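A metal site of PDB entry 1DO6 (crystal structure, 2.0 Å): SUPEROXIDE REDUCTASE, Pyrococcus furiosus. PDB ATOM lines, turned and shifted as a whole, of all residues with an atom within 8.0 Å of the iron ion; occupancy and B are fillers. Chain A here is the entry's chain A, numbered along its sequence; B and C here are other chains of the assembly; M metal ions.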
ATOM      1  N   TRP A  11     -20.669  -5.504 -15.010  1.00  0.00           N
ATOM      2  CA  TRP A  11     -19.425  -5.317 -14.263  1.00  0.00           C
ATOM      3  C   TRP A  11     -19.971  -5.480 -12.841  1.00  0.00           C
ATOM      4  O   TRP A  11     -21.196  -5.426 -12.642  1.00  0.00           O
ATOM      5  CB  TRP A  11     -18.811  -3.923 -14.479  1.00  0.00           C
ATOM      6  CG  TRP A  11     -19.673  -2.728 -14.180  1.00  0.00           C
ATOM      7  CD1 TRP A  11     -19.953  -2.210 -12.943  1.00  0.00           C
ATOM      8  CD2 TRP A  11     -20.300  -1.854 -15.134  1.00  0.00           C
ATOM      9  NE1 TRP A  11     -20.712  -1.059 -13.075  1.00  0.00           N
ATOM     10  CE2 TRP A  11     -20.940  -0.833 -14.411  1.00  0.00           C
ATOM     11  CE3 TRP A  11     -20.380  -1.851 -16.534  1.00  0.00           C
ATOM     12  CZ2 TRP A  11     -21.654   0.204 -15.041  1.00  0.00           C
ATOM     13  CZ3 TRP A  11     -21.088  -0.826 -17.160  1.00  0.00           C
ATOM     14  CH2 TRP A  11     -21.720   0.188 -16.411  1.00  0.00           C
ATOM     15  N   GLU A  14     -23.298  -3.089 -10.411  1.00  0.00           N
ATOM     16  CA  GLU A  14     -24.543  -2.606 -11.028  1.00  0.00           C
ATOM     17  C   GLU A  14     -25.045  -3.618 -12.083  1.00  0.00           C
ATOM     18  O   GLU A  14     -24.296  -4.025 -12.985  1.00  0.00           O
ATOM     19  CB  GLU A  14     -24.341  -1.231 -11.671  1.00  0.00           C
ATOM     20  CG  GLU A  14     -25.628  -0.679 -12.321  1.00  0.00           C
ATOM     21  CD  GLU A  14     -25.564   0.810 -12.605  1.00  0.00           C
ATOM     22  OE1 GLU A  14     -24.734   1.498 -11.989  1.00  0.00           O
ATOM     23  OE2 GLU A  14     -26.345   1.284 -13.456  1.00  0.00           O
ATOM     24  N   LYS A  15     -26.316  -4.002 -11.978  1.00  0.00           N
ATOM     25  CA  LYS A  15     -26.885  -4.990 -12.895  1.00  0.00           C
ATOM     26  C   LYS A  15     -27.637  -4.332 -14.051  1.00  0.00           C
ATOM     27  O   LYS A  15     -28.569  -3.575 -13.839  1.00  0.00           O
ATOM     28  CB  LYS A  15     -27.835  -5.938 -12.144  1.00  0.00           C
ATOM     29  CG  LYS A  15     -27.217  -6.600 -10.920  1.00  0.00           C
ATOM     30  CD  LYS A  15     -27.158  -8.120 -11.047  1.00  0.00           C
ATOM     31  CE  LYS A  15     -25.732  -8.653 -10.854  1.00  0.00           C
ATOM     32  NZ  LYS A  15     -25.128  -9.179 -12.133  1.00  0.00           N
ATOM     33  N   HIS A  16     -27.181  -4.619 -15.264  1.00  0.00           N
ATOM     34  CA  HIS A  16     -27.812  -4.073 -16.465  1.00  0.00           C
ATOM     35  C   HIS A  16     -28.375  -5.181 -17.374  1.00  0.00           C
ATOM     36  O   HIS A  16     -29.317  -4.941 -18.125  1.00  0.00           O
ATOM     37  CB  HIS A  16     -26.801  -3.288 -17.279  1.00  0.00           C
ATOM     38  CG  HIS A  16     -26.445  -1.965 -16.683  1.00  0.00           C
ATOM     39  ND1 HIS A  16     -25.211  -1.679 -16.152  1.00  0.00           N
ATOM     40  CD2 HIS A  16     -27.165  -0.817 -16.608  1.00  0.00           C
ATOM     41  CE1 HIS A  16     -25.219  -0.386 -15.768  1.00  0.00           C
ATOM     42  NE2 HIS A  16     -26.384   0.177 -16.029  1.00  0.00           N
ATOM     43  N   VAL A  35     -34.606  -6.184 -15.199  1.00  0.00           N
ATOM     44  CA  VAL A  35     -33.237  -5.761 -14.955  1.00  0.00           C
ATOM     45  C   VAL A  35     -33.086  -5.614 -13.445  1.00  0.00           C
ATOM     46  O   VAL A  35     -33.941  -5.044 -12.784  1.00  0.00           O
ATOM     47  CB  VAL A  35     -32.937  -4.399 -15.592  1.00  0.00           C
ATOM     48  CG1 VAL A  35     -31.557  -3.922 -15.151  1.00  0.00           C
ATOM     49  CG2 VAL A  35     -32.946  -4.531 -17.110  1.00  0.00           C
ATOM     50  N   HIS A  41     -31.204  -2.172  -9.978  1.00  0.00           N
ATOM     51  CA  HIS A  41     -30.496  -1.145 -10.688  1.00  0.00           C
ATOM     52  C   HIS A  41     -31.145   0.153 -10.186  1.00  0.00           C
ATOM     53  O   HIS A  41     -32.334   0.170  -9.817  1.00  0.00           O
ATOM     54  CB  HIS A  41     -30.729  -1.281 -12.187  1.00  0.00           C
ATOM     55  CG  HIS A  41     -30.148  -0.155 -12.989  1.00  0.00           C
ATOM     56  ND1 HIS A  41     -30.739   1.082 -13.134  1.00  0.00           N
ATOM     57  CD2 HIS A  41     -28.999  -0.103 -13.706  1.00  0.00           C
ATOM     58  CE1 HIS A  41     -29.950   1.815 -13.933  1.00  0.00           C
ATOM     59  NE2 HIS A  41     -28.880   1.131 -14.290  1.00  0.00           N
ATOM     60  N   PRO A  42     -30.376   1.248 -10.122  1.00  0.00           N
ATOM     61  CA  PRO A  42     -31.013   2.473  -9.647  1.00  0.00           C
ATOM     62  C   PRO A  42     -32.216   2.906 -10.498  1.00  0.00           C
ATOM     63  O   PRO A  42     -32.302   2.628 -11.703  1.00  0.00           O
ATOM     64  CB  PRO A  42     -29.897   3.523  -9.716  1.00  0.00           C
ATOM     65  CG  PRO A  42     -28.621   2.731  -9.765  1.00  0.00           C
ATOM     66  CD  PRO A  42     -28.950   1.432 -10.430  1.00  0.00           C
ATOM     67  N   HIS A  47     -30.743   8.608 -13.384  1.00  0.00           N
ATOM     68  CA  HIS A  47     -30.183   7.308 -13.755  1.00  0.00           C
ATOM     69  C   HIS A  47     -31.248   6.254 -13.627  1.00  0.00           C
ATOM     70  O   HIS A  47     -31.678   5.903 -12.513  1.00  0.00           O
ATOM     71  CB  HIS A  47     -29.027   6.982 -12.806  1.00  0.00           C
ATOM     72  CG  HIS A  47     -28.330   5.709 -13.128  1.00  0.00           C
ATOM     73  ND1 HIS A  47     -27.472   5.051 -12.266  1.00  0.00           N
ATOM     74  CD2 HIS A  47     -28.365   4.953 -14.268  1.00  0.00           C
ATOM     75  CE1 HIS A  47     -27.036   3.946 -12.882  1.00  0.00           C
ATOM     76  NE2 HIS A  47     -27.556   3.861 -14.099  1.00  0.00           N
ATOM     77  N   HIS A  48     -31.657   5.688 -14.759  1.00  0.00           N
ATOM     78  CA  HIS A  48     -32.726   4.692 -14.707  1.00  0.00           C
ATOM     79  C   HIS A  48     -32.781   3.853 -15.987  1.00  0.00           C
ATOM     80  O   HIS A  48     -32.221   4.237 -17.017  1.00  0.00           O
ATOM     81  CB  HIS A  48     -34.051   5.450 -14.561  1.00  0.00           C
ATOM     82  CG  HIS A  48     -34.234   6.525 -15.591  1.00  0.00           C
ATOM     83  ND1 HIS A  48     -34.127   7.863 -15.297  1.00  0.00           N
ATOM     84  CD2 HIS A  48     -34.515   6.451 -16.919  1.00  0.00           C
ATOM     85  CE1 HIS A  48     -34.324   8.574 -16.389  1.00  0.00           C
ATOM     86  NE2 HIS A  48     -34.560   7.740 -17.398  1.00  0.00           N
ATOM     87  N   ILE A  49     -33.488   2.728 -15.925  1.00  0.00           N
ATOM     88  CA  ILE A  49     -33.692   1.870 -17.114  1.00  0.00           C
ATOM     89  C   ILE A  49     -34.874   2.466 -17.904  1.00  0.00           C
ATOM     90  O   ILE A  49     -35.964   2.629 -17.358  1.00  0.00           O
ATOM     91  CB  ILE A  49     -34.046   0.416 -16.700  1.00  0.00           C
ATOM     92  CG1 ILE A  49     -32.864  -0.224 -15.927  1.00  0.00           C
ATOM     93  CG2 ILE A  49     -34.385  -0.434 -17.992  1.00  0.00           C
ATOM     94  CD1 ILE A  49     -31.508  -0.038 -16.622  1.00  0.00           C
ATOM     95  N   TYR A 110     -32.004  -0.647 -22.211  1.00  0.00           N
ATOM     96  CA  TYR A 110     -31.278   0.616 -22.315  1.00  0.00           C
ATOM     97  C   TYR A 110     -31.275   1.397 -20.995  1.00  0.00           C
ATOM     98  O   TYR A 110     -32.326   1.708 -20.442  1.00  0.00           O
ATOM     99  CB  TYR A 110     -31.902   1.487 -23.407  1.00  0.00           C
ATOM    100  CG  TYR A 110     -31.234   2.831 -23.596  1.00  0.00           C
ATOM    101  CD1 TYR A 110     -29.943   2.933 -24.148  1.00  0.00           C
ATOM    102  CD2 TYR A 110     -31.889   4.008 -23.225  1.00  0.00           C
ATOM    103  CE1 TYR A 110     -29.333   4.178 -24.328  1.00  0.00           C
ATOM    104  CE2 TYR A 110     -31.280   5.263 -23.396  1.00  0.00           C
ATOM    105  CZ  TYR A 110     -30.001   5.329 -23.944  1.00  0.00           C
ATOM    106  OH  TYR A 110     -29.422   6.554 -24.097  1.00  0.00           O
ATOM    107  N   CYS A 111     -30.084   1.671 -20.477  1.00  0.00           N
ATOM    108  CA  CYS A 111     -29.932   2.462 -19.258  1.00  0.00           C
ATOM    109  C   CYS A 111     -29.655   3.876 -19.802  1.00  0.00           C
ATOM    110  O   CYS A 111     -28.879   4.020 -20.722  1.00  0.00           O
ATOM    111  CB  CYS A 111     -28.764   1.930 -18.434  1.00  0.00           C
ATOM    112  SG  CYS A 111     -28.295   3.011 -17.015  1.00  0.00           S
ATOM    113  N   ASN A 112     -30.277   4.911 -19.239  1.00  0.00           N
ATOM    114  CA  ASN A 112     -30.076   6.242 -19.809  1.00  0.00           C
ATOM    115  C   ASN A 112     -28.636   6.755 -19.821  1.00  0.00           C
ATOM    116  O   ASN A 112     -28.312   7.606 -20.633  1.00  0.00           O
ATOM    117  CB  ASN A 112     -31.000   7.278 -19.143  1.00  0.00           C
ATOM    118  CG  ASN A 112     -30.626   7.574 -17.693  1.00  0.00           C
ATOM    119  OD1 ASN A 112     -30.140   6.712 -16.974  1.00  0.00           O
ATOM    120  ND2 ASN A 112     -30.857   8.797 -17.268  1.00  0.00           N
ATOM    121  N   ILE A 113     -27.767   6.222 -18.971  1.00  0.00           N
ATOM    122  CA  ILE A 113     -26.373   6.671 -18.977  1.00  0.00           C
ATOM    123  C   ILE A 113     -25.374   5.540 -19.234  1.00  0.00           C
ATOM    124  O   ILE A 113     -24.184   5.801 -19.396  1.00  0.00           O
ATOM    125  CB  ILE A 113     -25.965   7.362 -17.621  1.00  0.00           C
ATOM    126  CG1 ILE A 113     -26.122   6.371 -16.475  1.00  0.00           C
ATOM    127  CG2 ILE A 113     -26.788   8.634 -17.421  1.00  0.00           C
ATOM    128  CD1 ILE A 113     -25.508   6.866 -15.131  1.00  0.00           C
ATOM    129  N   HIS A 114     -25.848   4.298 -19.258  1.00  0.00           N
ATOM    130  CA  HIS A 114     -24.961   3.156 -19.477  1.00  0.00           C
ATOM    131  C   HIS A 114     -25.163   2.359 -20.796  1.00  0.00           C
ATOM    132  O   HIS A 114     -24.793   1.187 -20.888  1.00  0.00           O
ATOM    133  CB  HIS A 114     -25.086   2.211 -18.284  1.00  0.00           C
ATOM    134  CG  HIS A 114     -24.552   2.778 -16.999  1.00  0.00           C
ATOM    135  ND1 HIS A 114     -25.246   2.658 -15.825  1.00  0.00           N
ATOM    136  CD2 HIS A 114     -23.379   3.415 -16.779  1.00  0.00           C
ATOM    137  CE1 HIS A 114     -24.487   3.230 -14.906  1.00  0.00           C
ATOM    138  NE2 HIS A 114     -23.340   3.703 -15.430  1.00  0.00           N
ATOM    139  N   GLY A 115     -25.748   3.003 -21.799  1.00  0.00           N
ATOM    140  CA  GLY A 115     -25.943   2.362 -23.100  1.00  0.00           C
ATOM    141  C   GLY A 115     -26.862   1.151 -23.178  1.00  0.00           C
ATOM    142  O   GLY A 115     -27.681   0.897 -22.284  1.00  0.00           O
ATOM    143  N   TRP A 117     -27.862  -2.974 -23.566  1.00  0.00           N
ATOM    144  CA  TRP A 117     -27.539  -4.273 -22.995  1.00  0.00           C
ATOM    145  C   TRP A 117     -28.414  -5.346 -23.649  1.00  0.00           C
ATOM    146  O   TRP A 117     -29.571  -5.093 -24.012  1.00  0.00           O
ATOM    147  CB  TRP A 117     -27.782  -4.250 -21.490  1.00  0.00           C
ATOM    148  CG  TRP A 117     -26.851  -3.265 -20.835  1.00  0.00           C
ATOM    149  CD1 TRP A 117     -26.968  -1.896 -20.786  1.00  0.00           C
ATOM    150  CD2 TRP A 117     -25.581  -3.579 -20.240  1.00  0.00           C
ATOM    151  NE1 TRP A 117     -25.850  -1.332 -20.212  1.00  0.00           N
ATOM    152  CE2 TRP A 117     -24.980  -2.347 -19.863  1.00  0.00           C
ATOM    153  CE3 TRP A 117     -24.900  -4.779 -19.991  1.00  0.00           C
ATOM    154  CZ2 TRP A 117     -23.720  -2.287 -19.248  1.00  0.00           C
ATOM    155  CZ3 TRP A 117     -23.648  -4.713 -19.373  1.00  0.00           C
ATOM    156  CH2 TRP A 117     -23.071  -3.470 -19.009  1.00  0.00           C
ATOM    157  N   VAL B  79     -22.754   9.623 -17.017  1.00  0.00           N
ATOM    158  CA  VAL B  79     -22.177   9.073 -15.809  1.00  0.00           C
ATOM    159  C   VAL B  79     -21.562  10.222 -14.973  1.00  0.00           C
ATOM    160  O   VAL B  79     -21.237  10.047 -13.804  1.00  0.00           O
ATOM    161  CB  VAL B  79     -21.050   8.067 -16.142  1.00  0.00           C
ATOM    162  CG1 VAL B  79     -21.642   6.757 -16.689  1.00  0.00           C
ATOM    163  CG2 VAL B  79     -20.097   8.691 -17.163  1.00  0.00           C
ATOM    164  N   PHE C  63     -20.298   4.843 -23.712  1.00  0.00           N
ATOM    165  CA  PHE C  63     -21.710   4.506 -23.728  1.00  0.00           C
ATOM    166  C   PHE C  63     -22.458   5.240 -24.800  1.00  0.00           C
ATOM    167  O   PHE C  63     -22.334   6.451 -24.954  1.00  0.00           O
ATOM    168  CB  PHE C  63     -22.315   4.782 -22.355  1.00  0.00           C
ATOM    169  CG  PHE C  63     -21.590   4.074 -21.232  1.00  0.00           C
ATOM    170  CD1 PHE C  63     -20.733   4.776 -20.379  1.00  0.00           C
ATOM    171  CD2 PHE C  63     -21.755   2.707 -21.049  1.00  0.00           C
ATOM    172  CE1 PHE C  63     -20.053   4.121 -19.352  1.00  0.00           C
ATOM    173  CE2 PHE C  63     -21.089   2.036 -20.030  1.00  0.00           C
ATOM    174  CZ  PHE C  63     -20.233   2.748 -19.166  1.00  0.00           C
HETATM  175 FE    FE M   1     -27.120   1.988 -15.175  1.00  0.00          FE
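The iron ion is bound by OE2 of Glu 14 (2.0 Å), ND1 of His 114 (2.1 Å), NE2 of His 16 (2.1 Å), NE2 of His 41 (2.1 Å), NE2 of His 47 (2.2 Å) and SG of Cys 111 (2.4 Å).
O of His 114 is in hydrogen-bond range of NE1 of Trp 117, 2.8 Å away. SG of Cys 111 lies close to N of Ile 113.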
